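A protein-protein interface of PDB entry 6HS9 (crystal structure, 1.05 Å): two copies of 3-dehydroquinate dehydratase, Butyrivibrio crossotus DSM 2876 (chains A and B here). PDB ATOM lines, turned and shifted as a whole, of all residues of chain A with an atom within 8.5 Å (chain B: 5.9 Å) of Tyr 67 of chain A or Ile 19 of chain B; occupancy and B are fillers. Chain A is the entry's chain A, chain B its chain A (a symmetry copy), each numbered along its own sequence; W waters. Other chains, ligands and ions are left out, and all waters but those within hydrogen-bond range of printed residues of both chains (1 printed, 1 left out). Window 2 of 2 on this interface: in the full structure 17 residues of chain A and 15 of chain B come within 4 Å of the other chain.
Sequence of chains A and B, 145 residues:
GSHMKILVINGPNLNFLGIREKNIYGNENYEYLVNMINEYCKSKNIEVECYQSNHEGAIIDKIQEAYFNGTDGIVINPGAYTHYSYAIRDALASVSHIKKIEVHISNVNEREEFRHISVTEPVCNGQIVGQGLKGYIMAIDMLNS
The side-chain amide oxygen (OD1) of Asn 15 of chain B lies within hydrogen-bond range of the side-chain amide nitrogen (NE2) of Gln 64 of chain A.
O of Ala 91 of chain A lies within hydrogen-bond range of OG of Ser 94 of chain A (2.7 Å).
Phe 16 of chain B touches Gln 64 of chain A. CB of Tyr 67 of chain A touches CE2 of Phe 16 of chain B (3.9 Å). CE1 of Tyr 67 of chain A touches CG2 of Ile 19 of chain B, at 3.6 Å. Phe 68 of chain A touches Phe 16 of chain B (CE2 to CZ, 3.7 Å). Ala 93 of chain A touches Glu 21 of chain B. Ser 94 of chain A touches Phe 16 of chain B. O of Ser 94 of chain A touches CG2 of Ile 19 of chain B, 3.9 Å away. Ser 94 of chain A touches Arg 20 of chain B.
Of chain B, only Phe 16 and Ile 19 come within 4 Å of Tyr 67 of chain A. Of chain A, only Tyr 67 and Ser 94 come within 4 Å of Ile 19 of chain B. No residue of chain A comes within 4 Å of Gly 18 of chain B. Of the printed residues of chain B, Gln 64 of chain A touches Asn 15 (2.9 Å) and Phe 16 (3.6 Å). Of the printed residues of chain A, Glu 21 of chain B touches Ala 93. Of the printed residues of chain B, Ala 93 of chain A touches Glu 21. Asp 72 of chain A touches none of the printed residues of chain B. Glu 28 of chain B touches none of the printed residues of chain A. The nearest printed residue of chain B that does not touch Tyr 67 of chain A is Gly 18 of chain B (6.5 Å).
Printed residues of chain A that touch a printed residue of chain B: Gln 64, Tyr 67, Phe 68, Ala 93 and Ser 94. Hydrophobic or aromatic side chains of chain A within 4 Å of the printed part of chain B: Tyr 67, Phe 68 and Ala 93. Of the 11 printed residues of chain B, 5 touch a printed residue of chain A. Along chain B the printed residues that touch a printed residue of chain A span positions 15 to 21. Among the printed residues, no Asp or Glu carboxylate lies within 4 Å of a Lys or Arg side-chain nitrogen of the other chain.
No position is printed for both chains.
Water W1 lies within hydrogen-bond range of the backbone carbonyl oxygen of Ala 93 of chain A (2.9 Å) and the backbone NH of Glu 21 of chain B (2.9 Å).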
ATOM      1  N   LEU A   7      13.778  -2.258   4.363  1.00  0.00           N
ATOM      2  CA  LEU A   7      13.927  -1.587   5.635  1.00  0.00           C
ATOM      3  C   LEU A   7      13.420  -2.496   6.758  1.00  0.00           C
ATOM      4  O   LEU A   7      12.275  -2.940   6.680  1.00  0.00           O
ATOM      5  CB  LEU A   7      13.086  -0.301   5.611  1.00  0.00           C
ATOM      6  CG  LEU A   7      13.002   0.457   6.934  1.00  0.00           C
ATOM      7  CD1 LEU A   7      14.360   0.990   7.412  1.00  0.00           C
ATOM      8  CD2 LEU A   7      11.987   1.583   6.819  1.00  0.00           C
ATOM      9  N   ILE A  60       6.795   6.142  12.513  1.00  0.00           N
ATOM     10  CA  ILE A  60       5.958   6.651  11.447  1.00  0.00           C
ATOM     11  C   ILE A  60       6.767   7.479  10.469  1.00  0.00           C
ATOM     12  O   ILE A  60       6.626   7.316   9.253  1.00  0.00           O
ATOM     13  CB  ILE A  60       4.769   7.442  12.044  1.00  0.00           C
ATOM     14  CG1 ILE A  60       3.893   6.516  12.888  1.00  0.00           C
ATOM     15  CG2 ILE A  60       3.998   8.142  10.915  1.00  0.00           C
ATOM     16  CD1 ILE A  60       2.863   7.217  13.730  1.00  0.00           C
ATOM     17  N   ASP A  61       7.618   8.368  10.998  1.00  0.00           N
ATOM     18  CA  ASP A  61       8.489   9.140  10.114  1.00  0.00           C
ATOM     19  C   ASP A  61       9.300   8.232   9.195  1.00  0.00           C
ATOM     20  O   ASP A  61       9.500   8.532   8.024  1.00  0.00           O
ATOM     21  CB  ASP A  61       9.443  10.021  10.926  1.00  0.00           C
ATOM     22  CG  ASP A  61       8.857  11.148  11.750  1.00  0.00           C
ATOM     23  OD1 ASP A  61       7.714  11.548  11.521  1.00  0.00           O
ATOM     24  OD2 ASP A  61       9.606  11.633  12.648  1.00  0.00           O
ATOM     25  N   LYS A  62       9.846   7.142   9.757  1.00  0.00           N
ATOM     26  CA  LYS A  62      10.713   6.275   8.972  1.00  0.00           C
ATOM     27  C   LYS A  62       9.922   5.524   7.880  1.00  0.00           C
ATOM     28  O   LYS A  62      10.438   5.332   6.769  1.00  0.00           O
ATOM     29  CB  LYS A  62      11.412   5.284   9.927  1.00  0.00           C
ATOM     30  CG  LYS A  62      12.597   4.595   9.320  1.00  0.00           C
ATOM     31  CD  LYS A  62      13.798   5.477   9.092  1.00  0.00           C
ATOM     32  CE  LYS A  62      14.992   4.710   8.529  1.00  0.00           C
ATOM     33  NZ  LYS A  62      16.093   5.604   8.197  1.00  0.00           N
ATOM     34  N   ILE A  63       8.689   5.128   8.195  1.00  0.00           N
ATOM     35  CA  ILE A  63       7.822   4.515   7.191  1.00  0.00           C
ATOM     36  C   ILE A  63       7.544   5.519   6.081  1.00  0.00           C
ATOM     37  O   ILE A  63       7.606   5.161   4.892  1.00  0.00           O
ATOM     38  CB  ILE A  63       6.524   4.020   7.867  1.00  0.00           C
ATOM     39  CG1 ILE A  63       6.806   2.850   8.820  1.00  0.00           C
ATOM     40  CG2 ILE A  63       5.509   3.618   6.796  1.00  0.00           C
ATOM     41  CD1 ILE A  63       5.670   2.587   9.785  1.00  0.00           C
ATOM     42  N   GLN A  64       7.264   6.757   6.431  1.00  0.00           N
ATOM     43  CA  GLN A  64       7.020   7.782   5.414  1.00  0.00           C
ATOM     44  C   GLN A  64       8.262   7.994   4.561  1.00  0.00           C
ATOM     45  O   GLN A  64       8.172   8.186   3.327  1.00  0.00           O
ATOM     46  CB  GLN A  64       6.540   9.062   6.063  1.00  0.00           C
ATOM     47  CG  GLN A  64       5.189   8.972   6.674  1.00  0.00           C
ATOM     48  CD  GLN A  64       4.670  10.274   7.202  1.00  0.00           C
ATOM     49  OE1 GLN A  64       5.443  11.164   7.615  1.00  0.00           O
ATOM     50  NE2 GLN A  64       3.366  10.409   7.237  1.00  0.00           N
ATOM     51  N   GLU A  65       9.450   8.051   5.180  1.00  0.00           N
ATOM     52  CA  GLU A  65      10.634   8.245   4.392  1.00  0.00           C
ATOM     53  C   GLU A  65      10.814   7.124   3.367  1.00  0.00           C
ATOM     54  O   GLU A  65      11.353   7.335   2.259  1.00  0.00           O
ATOM     55  CB  GLU A  65      11.839   8.392   5.314  1.00  0.00           C
ATOM     56  CG  GLU A  65      11.791   9.678   6.162  1.00  0.00           C
ATOM     57  CD  GLU A  65      12.626   9.757   7.404  1.00  0.00           C
ATOM     58  OE1 GLU A  65      13.440   8.830   7.658  1.00  0.00           O
ATOM     59  OE2 GLU A  65      12.450  10.786   8.154  1.00  0.00           O
ATOM     60  N   ALA A  66      10.414   5.889   3.721  1.00  0.00           N
ATOM     61  CA  ALA A  66      10.525   4.757   2.838  1.00  0.00           C
ATOM     62  C   ALA A  66       9.708   4.931   1.564  1.00  0.00           C
ATOM     63  O   ALA A  66      10.062   4.369   0.517  1.00  0.00           O
ATOM     64  CB  ALA A  66      10.122   3.497   3.544  1.00  0.00           C
ATOM     65  N   TYR A  67       8.618   5.685   1.617  1.00  0.00           N
ATOM     66  CA  TYR A  67       7.850   6.026   0.431  1.00  0.00           C
ATOM     67  C   TYR A  67       8.688   6.738  -0.604  1.00  0.00           C
ATOM     68  O   TYR A  67       8.515   6.491  -1.794  1.00  0.00           O
ATOM     69  CB  TYR A  67       6.608   6.854   0.834  1.00  0.00           C
ATOM     70  CG  TYR A  67       5.799   7.416  -0.324  1.00  0.00           C
ATOM     71  CD1 TYR A  67       4.834   6.680  -0.960  1.00  0.00           C
ATOM     72  CD2 TYR A  67       6.030   8.689  -0.773  1.00  0.00           C
ATOM     73  CE1 TYR A  67       4.121   7.218  -2.023  1.00  0.00           C
ATOM     74  CE2 TYR A  67       5.371   9.238  -1.837  1.00  0.00           C
ATOM     75  CZ  TYR A  67       4.376   8.498  -2.447  1.00  0.00           C
ATOM     76  OH  TYR A  67       3.705   9.065  -3.507  1.00  0.00           O
ATOM     77  N   PHE A  68       9.517   7.668  -0.183  1.00  0.00           N
ATOM     78  CA  PHE A  68      10.241   8.544  -1.097  1.00  0.00           C
ATOM     79  C   PHE A  68      11.565   7.962  -1.598  1.00  0.00           C
ATOM     80  O   PHE A  68      12.064   8.476  -2.578  1.00  0.00           O
ATOM     81  CB  PHE A  68      10.498   9.895  -0.457  1.00  0.00           C
ATOM     82  CG  PHE A  68       9.246  10.623  -0.076  1.00  0.00           C
ATOM     83  CD1 PHE A  68       8.497  11.291  -1.013  1.00  0.00           C
ATOM     84  CD2 PHE A  68       8.861  10.705   1.248  1.00  0.00           C
ATOM     85  CE1 PHE A  68       7.378  12.034  -0.636  1.00  0.00           C
ATOM     86  CE2 PHE A  68       7.750  11.427   1.630  1.00  0.00           C
ATOM     87  CZ  PHE A  68       7.025  12.079   0.708  1.00  0.00           C
ATOM     88  N   ASN A  69      12.107   6.942  -0.947  1.00  0.00           N
ATOM     89  CA  ASN A  69      13.482   6.543  -1.161  1.00  0.00           C
ATOM     90  C   ASN A  69      13.627   5.185  -1.850  1.00  0.00           C
ATOM     91  O   ASN A  69      14.713   4.579  -1.817  1.00  0.00           O
ATOM     92  CB  ASN A  69      14.307   6.588   0.091  1.00  0.00           C
ATOM     93  CG  ASN A  69      13.965   5.469   1.046  1.00  0.00           C
ATOM     94  OD1 ASN A  69      13.156   4.615   0.723  1.00  0.00           O
ATOM     95  ND2 ASN A  69      14.547   5.517   2.202  1.00  0.00           N
ATOM     96  N   GLY A  70      12.593   4.718  -2.451  1.00  0.00           N
ATOM     97  CA  GLY A  70      12.625   3.515  -3.247  1.00  0.00           C
ATOM     98  C   GLY A  70      12.637   2.215  -2.498  1.00  0.00           C
ATOM     99  O   GLY A  70      12.907   1.159  -3.086  1.00  0.00           O
ATOM    100  N   THR A  71      12.198   2.266  -1.232  1.00  0.00           N
ATOM    101  CA  THR A  71      12.082   1.042  -0.461  1.00  0.00           C
ATOM    102  C   THR A  71      11.027   0.118  -1.060  1.00  0.00           C
ATOM    103  O   THR A  71       9.908   0.547  -1.358  1.00  0.00           O
ATOM    104  CB  THR A  71      11.775   1.353   1.003  1.00  0.00           C
ATOM    105  OG1 THR A  71      12.837   2.095   1.582  1.00  0.00           O
ATOM    106  CG2 THR A  71      11.530   0.120   1.818  1.00  0.00           C
ATOM    107  N   ASP A  72      11.370  -1.169  -1.216  1.00  0.00           N
ATOM    108  CA  ASP A  72      10.470  -2.161  -1.762  1.00  0.00           C
ATOM    109  C   ASP A  72       9.668  -2.895  -0.703  1.00  0.00           C
ATOM    110  O   ASP A  72       8.509  -3.301  -0.937  1.00  0.00           O
ATOM    111  CB  ASP A  72      11.297  -3.171  -2.596  1.00  0.00           C
ATOM    112  CG  ASP A  72      12.010  -2.523  -3.762  1.00  0.00           C
ATOM    113  OD1 ASP A  72      11.281  -1.876  -4.587  1.00  0.00           O
ATOM    114  OD2 ASP A  72      13.262  -2.589  -3.769  1.00  0.00           O
ATOM    115  N   ILE A  74       9.206  -3.645   3.804  1.00  0.00           N
ATOM    116  CA  ILE A  74       9.462  -3.343   5.204  1.00  0.00           C
ATOM    117  C   ILE A  74       9.233  -4.595   6.025  1.00  0.00           C
ATOM    118  O   ILE A  74       8.197  -5.261   5.852  1.00  0.00           O
ATOM    119  CB  ILE A  74       8.519  -2.221   5.709  1.00  0.00           C
ATOM    120  CG1 ILE A  74       8.906  -0.903   5.047  1.00  0.00           C
ATOM    121  CG2 ILE A  74       8.536  -2.127   7.220  1.00  0.00           C
ATOM    122  CD1 ILE A  74       7.892   0.220   5.225  1.00  0.00           C
ATOM    123  N   ALA A  91       0.074   4.466   9.223  1.00  0.00           N
ATOM    124  CA  ALA A  91       1.296   4.725   8.463  1.00  0.00           C
ATOM    125  C   ALA A  91       1.588   3.581   7.484  1.00  0.00           C
ATOM    126  O   ALA A  91       1.915   3.800   6.323  1.00  0.00           O
ATOM    127  CB  ALA A  91       2.458   4.954   9.377  1.00  0.00           C
ATOM    128  N   ALA A  93      -0.539   1.519   6.277  1.00  0.00           N
ATOM    129  CA  ALA A  93      -1.579   1.534   5.246  1.00  0.00           C
ATOM    130  C   ALA A  93      -1.330   2.631   4.220  1.00  0.00           C
ATOM    131  O   ALA A  93      -1.764   2.500   3.078  1.00  0.00           O
ATOM    132  CB  ALA A  93      -2.924   1.741   5.852  1.00  0.00           C
ATOM    133  N   SER A  94      -0.642   3.707   4.601  1.00  0.00           N
ATOM    134  CA  SER A  94      -0.411   4.846   3.714  1.00  0.00           C
ATOM    135  C   SER A  94       0.601   4.563   2.623  1.00  0.00           C
ATOM    136  O   SER A  94       0.646   5.337   1.670  1.00  0.00           O
ATOM    137  CB  SER A  94       0.020   6.040   4.502  1.00  0.00           C
ATOM    138  OG  SER A  94       1.366   6.010   4.911  1.00  0.00           O
ATOM    139  N   VAL A  95       1.412   3.506   2.770  1.00  0.00           N
ATOM    140  CA  VAL A  95       2.438   3.161   1.811  1.00  0.00           C
ATOM    141  C   VAL A  95       1.996   1.898   1.060  1.00  0.00           C
ATOM    142  O   VAL A  95       2.501   0.791   1.281  1.00  0.00           O
ATOM    143  CB  VAL A  95       3.830   3.105   2.447  1.00  0.00           C
ATOM    144  CG1 VAL A  95       4.286   4.503   2.832  1.00  0.00           C
ATOM    145  CG2 VAL A  95       3.948   2.143   3.615  1.00  0.00           C
ATOM    146  N   SER A  96       1.044   2.072   0.160  1.00  0.00           N
ATOM    147  CA  SER A  96       0.351   0.973  -0.468  1.00  0.00           C
ATOM    148  C   SER A  96       1.228   0.194  -1.441  1.00  0.00           C
ATOM    149  O   SER A  96       0.844  -0.895  -1.828  1.00  0.00           O
ATOM    150  CB  SER A  96      -0.915   1.392  -1.133  1.00  0.00           C
ATOM    151  OG  SER A  96      -0.621   2.371  -2.111  1.00  0.00           O
ATOM    152  N   HIS A  97       2.329   0.765  -1.890  1.00  0.00           N
ATOM    153  CA  HIS A  97       3.194   0.089  -2.836  1.00  0.00           C
ATOM    154  C   HIS A  97       4.412  -0.562  -2.191  1.00  0.00           C
ATOM    155  O   HIS A  97       5.293  -1.066  -2.892  1.00  0.00           O
ATOM    156  CB  HIS A  97       3.596   1.026  -3.953  1.00  0.00           C
ATOM    157  CG  HIS A  97       2.406   1.565  -4.690  1.00  0.00           C
ATOM    158  ND1 HIS A  97       1.660   0.842  -5.603  1.00  0.00           N
ATOM    159  CD2 HIS A  97       1.736   2.726  -4.531  1.00  0.00           C
ATOM    160  CE1 HIS A  97       0.663   1.565  -6.051  1.00  0.00           C
ATOM    161  NE2 HIS A  97       0.691   2.729  -5.408  1.00  0.00           N
ATOM    162  N   ILE A  98       4.455  -0.561  -0.876  1.00  0.00           N
ATOM    163  CA  ILE A  98       5.548  -1.173  -0.142  1.00  0.00           C
ATOM    164  C   ILE A  98       4.976  -2.420   0.513  1.00  0.00           C
ATOM    165  O   ILE A  98       4.001  -2.327   1.246  1.00  0.00           O
ATOM    166  CB  ILE A  98       6.148  -0.234   0.900  1.00  0.00           C
ATOM    167  CG1 ILE A  98       6.649   1.054   0.260  1.00  0.00           C
ATOM    168  CG2 ILE A  98       7.234  -0.952   1.683  1.00  0.00           C
ATOM    169  CD1 ILE A  98       7.352   2.005   1.241  1.00  0.00           C
ATOM    170  N   ASN B  15       0.185  14.506   6.990  1.00  0.00           N
ATOM    171  CA  ASN B  15       1.026  15.042   5.948  1.00  0.00           C
ATOM    172  C   ASN B  15       1.021  14.179   4.694  1.00  0.00           C
ATOM    173  O   ASN B  15       1.561  14.630   3.674  1.00  0.00           O
ATOM    174  CB  ASN B  15       2.452  15.215   6.470  1.00  0.00           C
ATOM    175  CG  ASN B  15       3.042  13.916   6.968  1.00  0.00           C
ATOM    176  OD1 ASN B  15       2.414  13.116   7.635  1.00  0.00           O
ATOM    177  ND2 ASN B  15       4.321  13.716   6.704  1.00  0.00           N
ATOM    178  N   PHE B  16       0.464  12.982   4.725  1.00  0.00           N
ATOM    179  CA  PHE B  16       0.331  12.107   3.574  1.00  0.00           C
ATOM    180  C   PHE B  16      -1.030  12.174   2.922  1.00  0.00           C
ATOM    181  O   PHE B  16      -1.378  11.353   2.072  1.00  0.00           O
ATOM    182  CB  PHE B  16       0.764  10.672   3.899  1.00  0.00           C
ATOM    183  CG  PHE B  16       2.197  10.321   3.574  1.00  0.00           C
ATOM    184  CD1 PHE B  16       3.231  11.228   3.779  1.00  0.00           C
ATOM    185  CD2 PHE B  16       2.527   9.073   3.124  1.00  0.00           C
ATOM    186  CE1 PHE B  16       4.531  10.916   3.438  1.00  0.00           C
ATOM    187  CE2 PHE B  16       3.843   8.766   2.793  1.00  0.00           C
ATOM    188  CZ  PHE B  16       4.815   9.686   2.970  1.00  0.00           C
ATOM    189  N   LEU B  17      -1.822  13.220   3.223  1.00  0.00           N
ATOM    190  CA  LEU B  17      -3.019  13.452   2.423  1.00  0.00           C
ATOM    191  C   LEU B  17      -2.646  13.533   0.955  1.00  0.00           C
ATOM    192  O   LEU B  17      -1.611  14.024   0.559  1.00  0.00           O
ATOM    193  CB  LEU B  17      -3.649  14.773   2.836  1.00  0.00           C
ATOM    194  CG  LEU B  17      -4.421  14.721   4.118  1.00  0.00           C
ATOM    195  CD1 LEU B  17      -4.809  16.139   4.528  1.00  0.00           C
ATOM    196  CD2 LEU B  17      -5.655  13.866   4.020  1.00  0.00           C
ATOM    197  N   GLY B  18      -3.491  12.922   0.108  1.00  0.00           N
ATOM    198  CA  GLY B  18      -3.248  12.853  -1.344  1.00  0.00           C
ATOM    199  C   GLY B  18      -2.425  11.663  -1.800  1.00  0.00           C
ATOM    200  O   GLY B  18      -2.252  11.528  -2.995  1.00  0.00           O
ATOM    201  N   ILE B  19      -1.673  11.085  -0.898  1.00  0.00           N
ATOM    202  CA  ILE B  19      -0.915   9.864  -1.126  1.00  0.00           C
ATOM    203  C   ILE B  19      -1.715   8.736  -0.495  1.00  0.00           C
ATOM    204  O   ILE B  19      -1.961   7.705  -1.111  1.00  0.00           O
ATOM    205  CB  ILE B  19       0.478   9.958  -0.475  1.00  0.00           C
ATOM    206  CG1 ILE B  19       1.355  11.005  -1.130  1.00  0.00           C
ATOM    207  CG2 ILE B  19       1.160   8.586  -0.432  1.00  0.00           C
ATOM    208  CD1 ILE B  19       2.598  11.366  -0.342  1.00  0.00           C
ATOM    209  N   ARG B  20      -2.149   8.897   0.754  1.00  0.00           N
ATOM    210  CA  ARG B  20      -2.755   7.820   1.502  1.00  0.00           C
ATOM    211  C   ARG B  20      -4.200   7.667   1.054  1.00  0.00           C
ATOM    212  O   ARG B  20      -4.925   8.636   0.927  1.00  0.00           O
ATOM    213  CB  ARG B  20      -2.622   8.122   3.019  1.00  0.00           C
ATOM    214  CG  ARG B  20      -3.547   9.246   3.474  1.00  0.00           C
ATOM    215  CD  ARG B  20      -3.123   9.648   4.893  1.00  0.00           C
ATOM    216  NE  ARG B  20      -3.565   8.698   5.854  1.00  0.00           N
ATOM    217  CZ  ARG B  20      -4.158   9.000   6.988  1.00  0.00           C
ATOM    218  NH1 ARG B  20      -4.227  10.253   7.399  1.00  0.00           N
ATOM    219  NH2 ARG B  20      -4.561   8.043   7.775  1.00  0.00           N
ATOM    220  N   GLU B  21      -4.650   6.403   1.045  1.00  0.00           N
ATOM    221  CA  GLU B  21      -6.038   6.020   0.997  1.00  0.00           C
ATOM    222  C   GLU B  21      -6.967   7.086   0.402  1.00  0.00           C
ATOM    223  O   GLU B  21      -7.869   7.722   1.028  1.00  0.00           O
ATOM    224  CB  GLU B  21      -6.437   5.539   2.387  1.00  0.00           C
ATOM    225  CG  GLU B  21      -5.604   4.420   2.973  1.00  0.00           C
ATOM    226  CD  GLU B  21      -6.150   3.985   4.329  1.00  0.00           C
ATOM    227  OE1 GLU B  21      -5.693   4.571   5.338  1.00  0.00           O
ATOM    228  OE2 GLU B  21      -6.953   3.029   4.415  1.00  0.00           O
ATOM    229  N   LYS B  22      -6.854   7.296  -0.883  1.00  0.00           N
ATOM    230  CA  LYS B  22      -7.506   8.408  -1.587  1.00  0.00           C
ATOM    231  C   LYS B  22      -9.034   8.354  -1.612  1.00  0.00           C
ATOM    232  O   LYS B  22      -9.724   9.386  -1.631  1.00  0.00           O
ATOM    233  CB  LYS B  22      -6.926   8.638  -2.969  1.00  0.00           C
ATOM    234  CG  LYS B  22      -5.507   9.203  -3.045  1.00  0.00           C
ATOM    235  CD  LYS B  22      -4.817   8.807  -4.362  1.00  0.00           C
ATOM    236  CE  LYS B  22      -3.961   9.877  -5.026  1.00  0.00           C
ATOM    237  NZ  LYS B  22      -4.708  11.140  -5.212  1.00  0.00           N
ATOM    238  N   GLY B  26      -9.479  11.797   0.268  1.00  0.00           N
ATOM    239  CA  GLY B  26      -9.546  12.742  -0.822  1.00  0.00           C
ATOM    240  C   GLY B  26      -8.264  12.770  -1.660  1.00  0.00           C
ATOM    241  O   GLY B  26      -7.223  12.191  -1.324  1.00  0.00           O
ATOM    242  N   GLU B  28      -6.681  15.701  -2.685  1.00  0.00           N
ATOM    243  CA  GLU B  28      -5.836  16.854  -2.479  1.00  0.00           C
ATOM    244  C   GLU B  28      -4.818  16.580  -1.376  1.00  0.00           C
ATOM    245  O   GLU B  28      -5.063  15.795  -0.459  1.00  0.00           O
ATOM    246  CB  GLU B  28      -6.629  18.110  -2.171  1.00  0.00           C
ATOM    247  CG  GLU B  28      -7.638  18.485  -3.211  1.00  0.00           C
ATOM    248  CD  GLU B  28      -7.155  18.753  -4.604  1.00  0.00           C
ATOM    249  OE1 GLU B  28      -5.976  18.999  -4.856  1.00  0.00           O
ATOM    250  OE2 GLU B  28      -8.055  18.769  -5.498  1.00  0.00           O
ATOM    251  N   ASN B  29      -3.664  17.232  -1.486  1.00  0.00           N
ATOM    252  CA  ASN B  29      -2.528  16.952  -0.632  1.00  0.00           C
ATOM    253  C   ASN B  29      -2.494  17.898   0.567  1.00  0.00           C
ATOM    254  O   ASN B  29      -3.313  18.826   0.756  1.00  0.00           O
ATOM    255  CB  ASN B  29      -1.244  16.797  -1.407  1.00  0.00           C
ATOM    256  CG  ASN B  29      -0.778  18.081  -2.018  1.00  0.00           C
ATOM    257  OD1 ASN B  29      -1.156  19.189  -1.597  1.00  0.00           O
ATOM    258  ND2 ASN B  29       0.080  17.971  -3.038  1.00  0.00           N
HETATM  259  O   HOH W   1      -2.727   4.189   0.908  1.00  0.00           O
